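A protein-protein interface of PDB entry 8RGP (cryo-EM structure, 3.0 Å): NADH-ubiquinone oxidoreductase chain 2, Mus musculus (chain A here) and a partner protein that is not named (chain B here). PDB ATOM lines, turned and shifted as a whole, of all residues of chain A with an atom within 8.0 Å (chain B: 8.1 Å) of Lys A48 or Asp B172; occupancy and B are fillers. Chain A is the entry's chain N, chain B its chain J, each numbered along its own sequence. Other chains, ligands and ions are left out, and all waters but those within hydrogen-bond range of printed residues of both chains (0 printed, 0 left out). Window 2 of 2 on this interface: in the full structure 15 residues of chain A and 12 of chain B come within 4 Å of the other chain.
The guanidinium group (NH1) of Arg B171 sits at hydrogen-bond distance from O of FME A1. SD of FME A1 lies close to the side-chain carboxylate (OE1) of Glu B168, at 3.3 Å.
Among the printed residues, merely in contact across the chains: Ile A41 with Ile B169 (3.8 Å), Pro A42 with Ile B169 (3.9 Å), Lys A48 with Glu B168 (3.6 Å), Lys A48 with Ile B169 (3.6 Å) and Lys A48 with Asp B172 (3.6 Å).
Lys A48 touches just these residues of chain B: Glu B168, Ile B169 and Asp B172. Of the printed residues of chain A, Ile B169 touches Ile A41, Pro A42 and Lys A48. Of the printed residues of chain A, Arg B171 touches FME A1. Printed residues of chain B within 4 Å of Pro A42: Ile B169. Ile B167 touches none of the printed residues of chain A. Asn A46 touches none of the printed residues of chain B. The nearest residue of chain B that does not touch Lys A48 is Arg B171 (4.1 Å). The nearest residue of chain A that does not touch Asp B172 is Asn A46 (7.1 Å).
Hydrophobic or aromatic side chains of chain B that line the printed part of chain A: Ile B169. Of the 14 printed residues of chain A, 4 touch a printed residue of chain B.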
ATOM      1  N   FME A   1      -4.487 -25.567  14.113  1.00  0.00           N
ATOM      2  CN  FME A   1      -3.708 -26.353  13.300  1.00  0.00           C
ATOM      3  O1  FME A   1      -2.635 -25.976  12.808  1.00  0.00           O
ATOM      4  CA  FME A   1      -4.164 -24.221  14.490  1.00  0.00           C
ATOM      5  CB  FME A   1      -4.468 -23.199  13.382  1.00  0.00           C
ATOM      6  CG  FME A   1      -3.214 -22.736  12.696  1.00  0.00           C
ATOM      7  SD  FME A   1      -2.423 -21.651  13.841  1.00  0.00           S
ATOM      8  CE  FME A   1      -1.217 -20.873  12.843  1.00  0.00           C
ATOM      9  C   FME A   1      -4.934 -23.803  15.739  1.00  0.00           C
ATOM     10  O   FME A   1      -5.201 -24.589  16.648  1.00  0.00           O
ATOM     11  N   ILE A  41       6.302 -15.897   8.268  1.00  0.00           N
ATOM     12  CA  ILE A  41       7.062 -17.148   8.427  1.00  0.00           C
ATOM     13  C   ILE A  41       6.239 -18.310   8.998  1.00  0.00           C
ATOM     14  O   ILE A  41       6.281 -19.406   8.413  1.00  0.00           O
ATOM     15  CB  ILE A  41       8.359 -16.884   9.206  1.00  0.00           C
ATOM     16  CG1 ILE A  41       9.371 -16.204   8.296  1.00  0.00           C
ATOM     17  CG2 ILE A  41       8.949 -18.174   9.738  1.00  0.00           C
ATOM     18  CD1 ILE A  41      10.653 -15.887   8.971  1.00  0.00           C
ATOM     19  N   PRO A  42       5.484 -18.159  10.106  1.00  0.00           N
ATOM     20  CA  PRO A  42       4.702 -19.316  10.584  1.00  0.00           C
ATOM     21  C   PRO A  42       3.606 -19.747   9.636  1.00  0.00           C
ATOM     22  O   PRO A  42       3.213 -20.919   9.657  1.00  0.00           O
ATOM     23  CB  PRO A  42       4.109 -18.827  11.911  1.00  0.00           C
ATOM     24  CG  PRO A  42       4.908 -17.711  12.292  1.00  0.00           C
ATOM     25  CD  PRO A  42       5.323 -17.037  11.047  1.00  0.00           C
ATOM     26  N   LEU A  44       4.098 -19.782   6.446  1.00  0.00           N
ATOM     27  CA  LEU A  44       4.848 -20.613   5.512  1.00  0.00           C
ATOM     28  C   LEU A  44       5.072 -22.001   6.088  1.00  0.00           C
ATOM     29  O   LEU A  44       4.598 -22.998   5.535  1.00  0.00           O
ATOM     30  CB  LEU A  44       6.181 -19.952   5.162  1.00  0.00           C
ATOM     31  CG  LEU A  44       6.123 -18.638   4.386  1.00  0.00           C
ATOM     32  CD1 LEU A  44       7.511 -18.241   3.938  1.00  0.00           C
ATOM     33  CD2 LEU A  44       5.187 -18.745   3.199  1.00  0.00           C
ATOM     34  N   ILE A  45       5.752 -22.093   7.229  1.00  0.00           N
ATOM     35  CA  ILE A  45       6.009 -23.398   7.845  1.00  0.00           C
ATOM     36  C   ILE A  45       4.781 -23.729   8.692  1.00  0.00           C
ATOM     37  O   ILE A  45       4.667 -23.371   9.864  1.00  0.00           O
ATOM     38  CB  ILE A  45       7.328 -23.430   8.624  1.00  0.00           C
ATOM     39  CG1 ILE A  45       7.484 -24.746   9.392  1.00  0.00           C
ATOM     40  CG2 ILE A  45       7.532 -22.190   9.500  1.00  0.00           C
ATOM     41  CD1 ILE A  45       8.787 -24.859  10.123  1.00  0.00           C
ATOM     42  N   ASN A  46       3.832 -24.386   8.071  1.00  0.00           N
ATOM     43  CA  ASN A  46       2.613 -24.780   8.761  1.00  0.00           C
ATOM     44  C   ASN A  46       2.297 -26.254   8.587  1.00  0.00           C
ATOM     45  O   ASN A  46       1.738 -26.870   9.497  1.00  0.00           O
ATOM     46  CB  ASN A  46       1.436 -23.935   8.273  1.00  0.00           C
ATOM     47  CG  ASN A  46       0.201 -24.119   9.121  1.00  0.00           C
ATOM     48  OD1 ASN A  46       0.287 -24.512  10.281  1.00  0.00           O
ATOM     49  ND2 ASN A  46      -0.958 -23.829   8.549  1.00  0.00           N
ATOM     50  N   LYS A  47       2.634 -26.837   7.440  1.00  0.00           N
ATOM     51  CA  LYS A  47       2.410 -28.256   7.221  1.00  0.00           C
ATOM     52  C   LYS A  47       3.475 -29.131   7.862  1.00  0.00           C
ATOM     53  O   LYS A  47       3.261 -30.342   7.975  1.00  0.00           O
ATOM     54  CB  LYS A  47       2.333 -28.540   5.725  1.00  0.00           C
ATOM     55  CG  LYS A  47       1.047 -28.068   5.092  1.00  0.00           C
ATOM     56  CD  LYS A  47      -0.135 -28.806   5.692  1.00  0.00           C
ATOM     57  CE  LYS A  47      -1.168 -27.847   6.253  1.00  0.00           C
ATOM     58  NZ  LYS A  47      -2.293 -28.578   6.894  1.00  0.00           N
ATOM     59  N   LYS A  48       4.601 -28.541   8.275  1.00  0.00           N
ATOM     60  CA  LYS A  48       5.681 -29.228   8.989  1.00  0.00           C
ATOM     61  C   LYS A  48       6.248 -30.401   8.190  1.00  0.00           C
ATOM     62  O   LYS A  48       6.509 -31.475   8.731  1.00  0.00           O
ATOM     63  CB  LYS A  48       5.223 -29.683  10.376  1.00  0.00           C
ATOM     64  CG  LYS A  48       4.608 -28.574  11.208  1.00  0.00           C
ATOM     65  CD  LYS A  48       5.625 -27.500  11.538  1.00  0.00           C
ATOM     66  CE  LYS A  48       4.952 -26.283  12.141  1.00  0.00           C
ATOM     67  NZ  LYS A  48       4.040 -26.647  13.257  1.00  0.00           N
ATOM     68  N   ASN A  49       6.430 -30.199   6.900  1.00  0.00           N
ATOM     69  CA  ASN A  49       7.183 -31.127   6.075  1.00  0.00           C
ATOM     70  C   ASN A  49       8.587 -30.582   5.854  1.00  0.00           C
ATOM     71  O   ASN A  49       8.847 -29.408   6.131  1.00  0.00           O
ATOM     72  CB  ASN A  49       6.466 -31.352   4.735  1.00  0.00           C
ATOM     73  CG  ASN A  49       6.193 -30.073   3.991  1.00  0.00           C
ATOM     74  OD1 ASN A  49       7.096 -29.467   3.418  1.00  0.00           O
ATOM     75  ND2 ASN A  49       4.937 -29.662   3.972  1.00  0.00           N
ATOM     76  N   PRO A  50       9.541 -31.414   5.412  1.00  0.00           N
ATOM     77  CA  PRO A  50      10.893 -30.889   5.144  1.00  0.00           C
ATOM     78  C   PRO A  50      10.941 -29.784   4.105  1.00  0.00           C
ATOM     79  O   PRO A  50      11.770 -28.872   4.227  1.00  0.00           O
ATOM     80  CB  PRO A  50      11.653 -32.131   4.671  1.00  0.00           C
ATOM     81  CG  PRO A  50      10.993 -33.241   5.366  1.00  0.00           C
ATOM     82  CD  PRO A  50       9.540 -32.889   5.435  1.00  0.00           C
ATOM     83  N   ARG A  51      10.076 -29.830   3.094  1.00  0.00           N
ATOM     84  CA  ARG A  51      10.070 -28.779   2.083  1.00  0.00           C
ATOM     85  C   ARG A  51       9.581 -27.456   2.658  1.00  0.00           C
ATOM     86  O   ARG A  51      10.133 -26.397   2.341  1.00  0.00           O
ATOM     87  CB  ARG A  51       9.216 -29.211   0.895  1.00  0.00           C
ATOM     88  CG  ARG A  51       9.809 -30.389   0.158  1.00  0.00           C
ATOM     89  CD  ARG A  51       8.912 -30.894  -0.943  1.00  0.00           C
ATOM     90  NE  ARG A  51       9.607 -31.877  -1.761  1.00  0.00           N
ATOM     91  CZ  ARG A  51      10.287 -31.588  -2.862  1.00  0.00           C
ATOM     92  NH1 ARG A  51      10.357 -30.352  -3.324  1.00  0.00           N
ATOM     93  NH2 ARG A  51      10.910 -32.562  -3.515  1.00  0.00           N
ATOM     94  N   SER A  52       8.557 -27.500   3.515  1.00  0.00           N
ATOM     95  CA  SER A  52       8.080 -26.284   4.166  1.00  0.00           C
ATOM     96  C   SER A  52       9.140 -25.697   5.086  1.00  0.00           C
ATOM     97  O   SER A  52       9.323 -24.475   5.129  1.00  0.00           O
ATOM     98  CB  SER A  52       6.801 -26.571   4.945  1.00  0.00           C
ATOM     99  OG  SER A  52       5.765 -26.979   4.073  1.00  0.00           O
ATOM    100  N   THR A  53       9.853 -26.556   5.818  1.00  0.00           N
ATOM    101  CA  THR A  53      10.920 -26.088   6.695  1.00  0.00           C
ATOM    102  C   THR A  53      12.047 -25.446   5.899  1.00  0.00           C
ATOM    103  O   THR A  53      12.562 -24.385   6.281  1.00  0.00           O
ATOM    104  CB  THR A  53      11.449 -27.251   7.529  1.00  0.00           C
ATOM    105  OG1 THR A  53      10.355 -27.904   8.182  1.00  0.00           O
ATOM    106  CG2 THR A  53      12.423 -26.757   8.575  1.00  0.00           C
ATOM    107  N   GLY A 121       7.074 -26.074  -2.593  1.00  0.00           N
ATOM    108  CA  GLY A 121       7.112 -26.592  -1.242  1.00  0.00           C
ATOM    109  C   GLY A 121       6.295 -25.807  -0.245  1.00  0.00           C
ATOM    110  O   GLY A 121       6.493 -25.966   0.963  1.00  0.00           O
ATOM    111  N   ILE B 166       6.589 -17.847  17.653  1.00  0.00           N
ATOM    112  CA  ILE B 166       7.507 -18.917  18.033  1.00  0.00           C
ATOM    113  C   ILE B 166       6.744 -20.134  18.534  1.00  0.00           C
ATOM    114  O   ILE B 166       7.160 -21.274  18.278  1.00  0.00           O
ATOM    115  CB  ILE B 166       8.549 -18.429  19.055  1.00  0.00           C
ATOM    116  CG1 ILE B 166       7.876 -17.937  20.334  1.00  0.00           C
ATOM    117  CG2 ILE B 166       9.396 -17.344  18.435  1.00  0.00           C
ATOM    118  CD1 ILE B 166       8.756 -17.823  21.529  1.00  0.00           C
ATOM    119  N   ILE B 167       5.608 -19.931  19.220  1.00  0.00           N
ATOM    120  CA  ILE B 167       4.800 -21.079  19.628  1.00  0.00           C
ATOM    121  C   ILE B 167       4.273 -21.821  18.406  1.00  0.00           C
ATOM    122  O   ILE B 167       4.329 -23.057  18.341  1.00  0.00           O
ATOM    123  CB  ILE B 167       3.662 -20.635  20.561  1.00  0.00           C
ATOM    124  CG1 ILE B 167       4.230 -20.137  21.886  1.00  0.00           C
ATOM    125  CG2 ILE B 167       2.710 -21.781  20.826  1.00  0.00           C
ATOM    126  CD1 ILE B 167       3.178 -19.716  22.878  1.00  0.00           C
ATOM    127  N   GLU B 168       3.802 -21.086  17.397  1.00  0.00           N
ATOM    128  CA  GLU B 168       3.272 -21.761  16.218  1.00  0.00           C
ATOM    129  C   GLU B 168       4.356 -22.393  15.354  1.00  0.00           C
ATOM    130  O   GLU B 168       4.086 -23.389  14.676  1.00  0.00           O
ATOM    131  CB  GLU B 168       2.433 -20.797  15.387  1.00  0.00           C
ATOM    132  CG  GLU B 168       1.064 -20.566  15.980  1.00  0.00           C
ATOM    133  CD  GLU B 168       0.340 -21.865  16.298  1.00  0.00           C
ATOM    134  OE1 GLU B 168       0.274 -22.748  15.415  1.00  0.00           O
ATOM    135  OE2 GLU B 168      -0.161 -22.007  17.433  1.00  0.00           O
ATOM    136  N   ILE B 169       5.571 -21.846  15.348  1.00  0.00           N
ATOM    137  CA  ILE B 169       6.647 -22.483  14.595  1.00  0.00           C
ATOM    138  C   ILE B 169       7.079 -23.773  15.274  1.00  0.00           C
ATOM    139  O   ILE B 169       7.167 -24.828  14.637  1.00  0.00           O
ATOM    140  CB  ILE B 169       7.836 -21.526  14.408  1.00  0.00           C
ATOM    141  CG1 ILE B 169       7.464 -20.373  13.483  1.00  0.00           C
ATOM    142  CG2 ILE B 169       9.003 -22.271  13.809  1.00  0.00           C
ATOM    143  CD1 ILE B 169       8.583 -19.390  13.275  1.00  0.00           C
ATOM    144  N   THR B 170       7.329 -23.722  16.582  1.00  0.00           N
ATOM    145  CA  THR B 170       7.790 -24.898  17.304  1.00  0.00           C
ATOM    146  C   THR B 170       6.649 -25.726  17.874  1.00  0.00           C
ATOM    147  O   THR B 170       6.871 -26.491  18.818  1.00  0.00           O
ATOM    148  CB  THR B 170       8.740 -24.489  18.427  1.00  0.00           C
ATOM    149  OG1 THR B 170       8.059 -23.609  19.326  1.00  0.00           O
ATOM    150  CG2 THR B 170       9.949 -23.781  17.862  1.00  0.00           C
ATOM    151  N   ARG B 171       5.433 -25.570  17.341  1.00  0.00           N
ATOM    152  CA  ARG B 171       4.311 -26.382  17.802  1.00  0.00           C
ATOM    153  C   ARG B 171       4.543 -27.861  17.526  1.00  0.00           C
ATOM    154  O   ARG B 171       4.273 -28.705  18.391  1.00  0.00           O
ATOM    155  CB  ARG B 171       3.016 -25.909  17.144  1.00  0.00           C
ATOM    156  CG  ARG B 171       1.874 -26.891  17.269  1.00  0.00           C
ATOM    157  CD  ARG B 171       0.571 -26.313  16.773  1.00  0.00           C
ATOM    158  NE  ARG B 171      -0.361 -27.372  16.408  1.00  0.00           N
ATOM    159  CZ  ARG B 171      -1.674 -27.214  16.309  1.00  0.00           C
ATOM    160  NH1 ARG B 171      -2.250 -26.054  16.575  1.00  0.00           N
ATOM    161  NH2 ARG B 171      -2.425 -28.248  15.943  1.00  0.00           N
ATOM    162  N   ASP B 172       5.061 -28.185  16.340  1.00  0.00           N
ATOM    163  CA  ASP B 172       5.355 -29.555  15.904  1.00  0.00           C
ATOM    164  C   ASP B 172       4.112 -30.442  15.953  1.00  0.00           C
ATOM    165  O   ASP B 172       2.988 -29.958  15.822  1.00  0.00           O
ATOM    166  CB  ASP B 172       6.491 -30.161  16.745  1.00  0.00           C
ATOM    167  CG  ASP B 172       6.971 -31.503  16.219  1.00  0.00           C
ATOM    168  OD1 ASP B 172       6.272 -32.520  16.413  1.00  0.00           O
ATOM    169  OD2 ASP B 172       8.062 -31.539  15.611  1.00  0.00           O
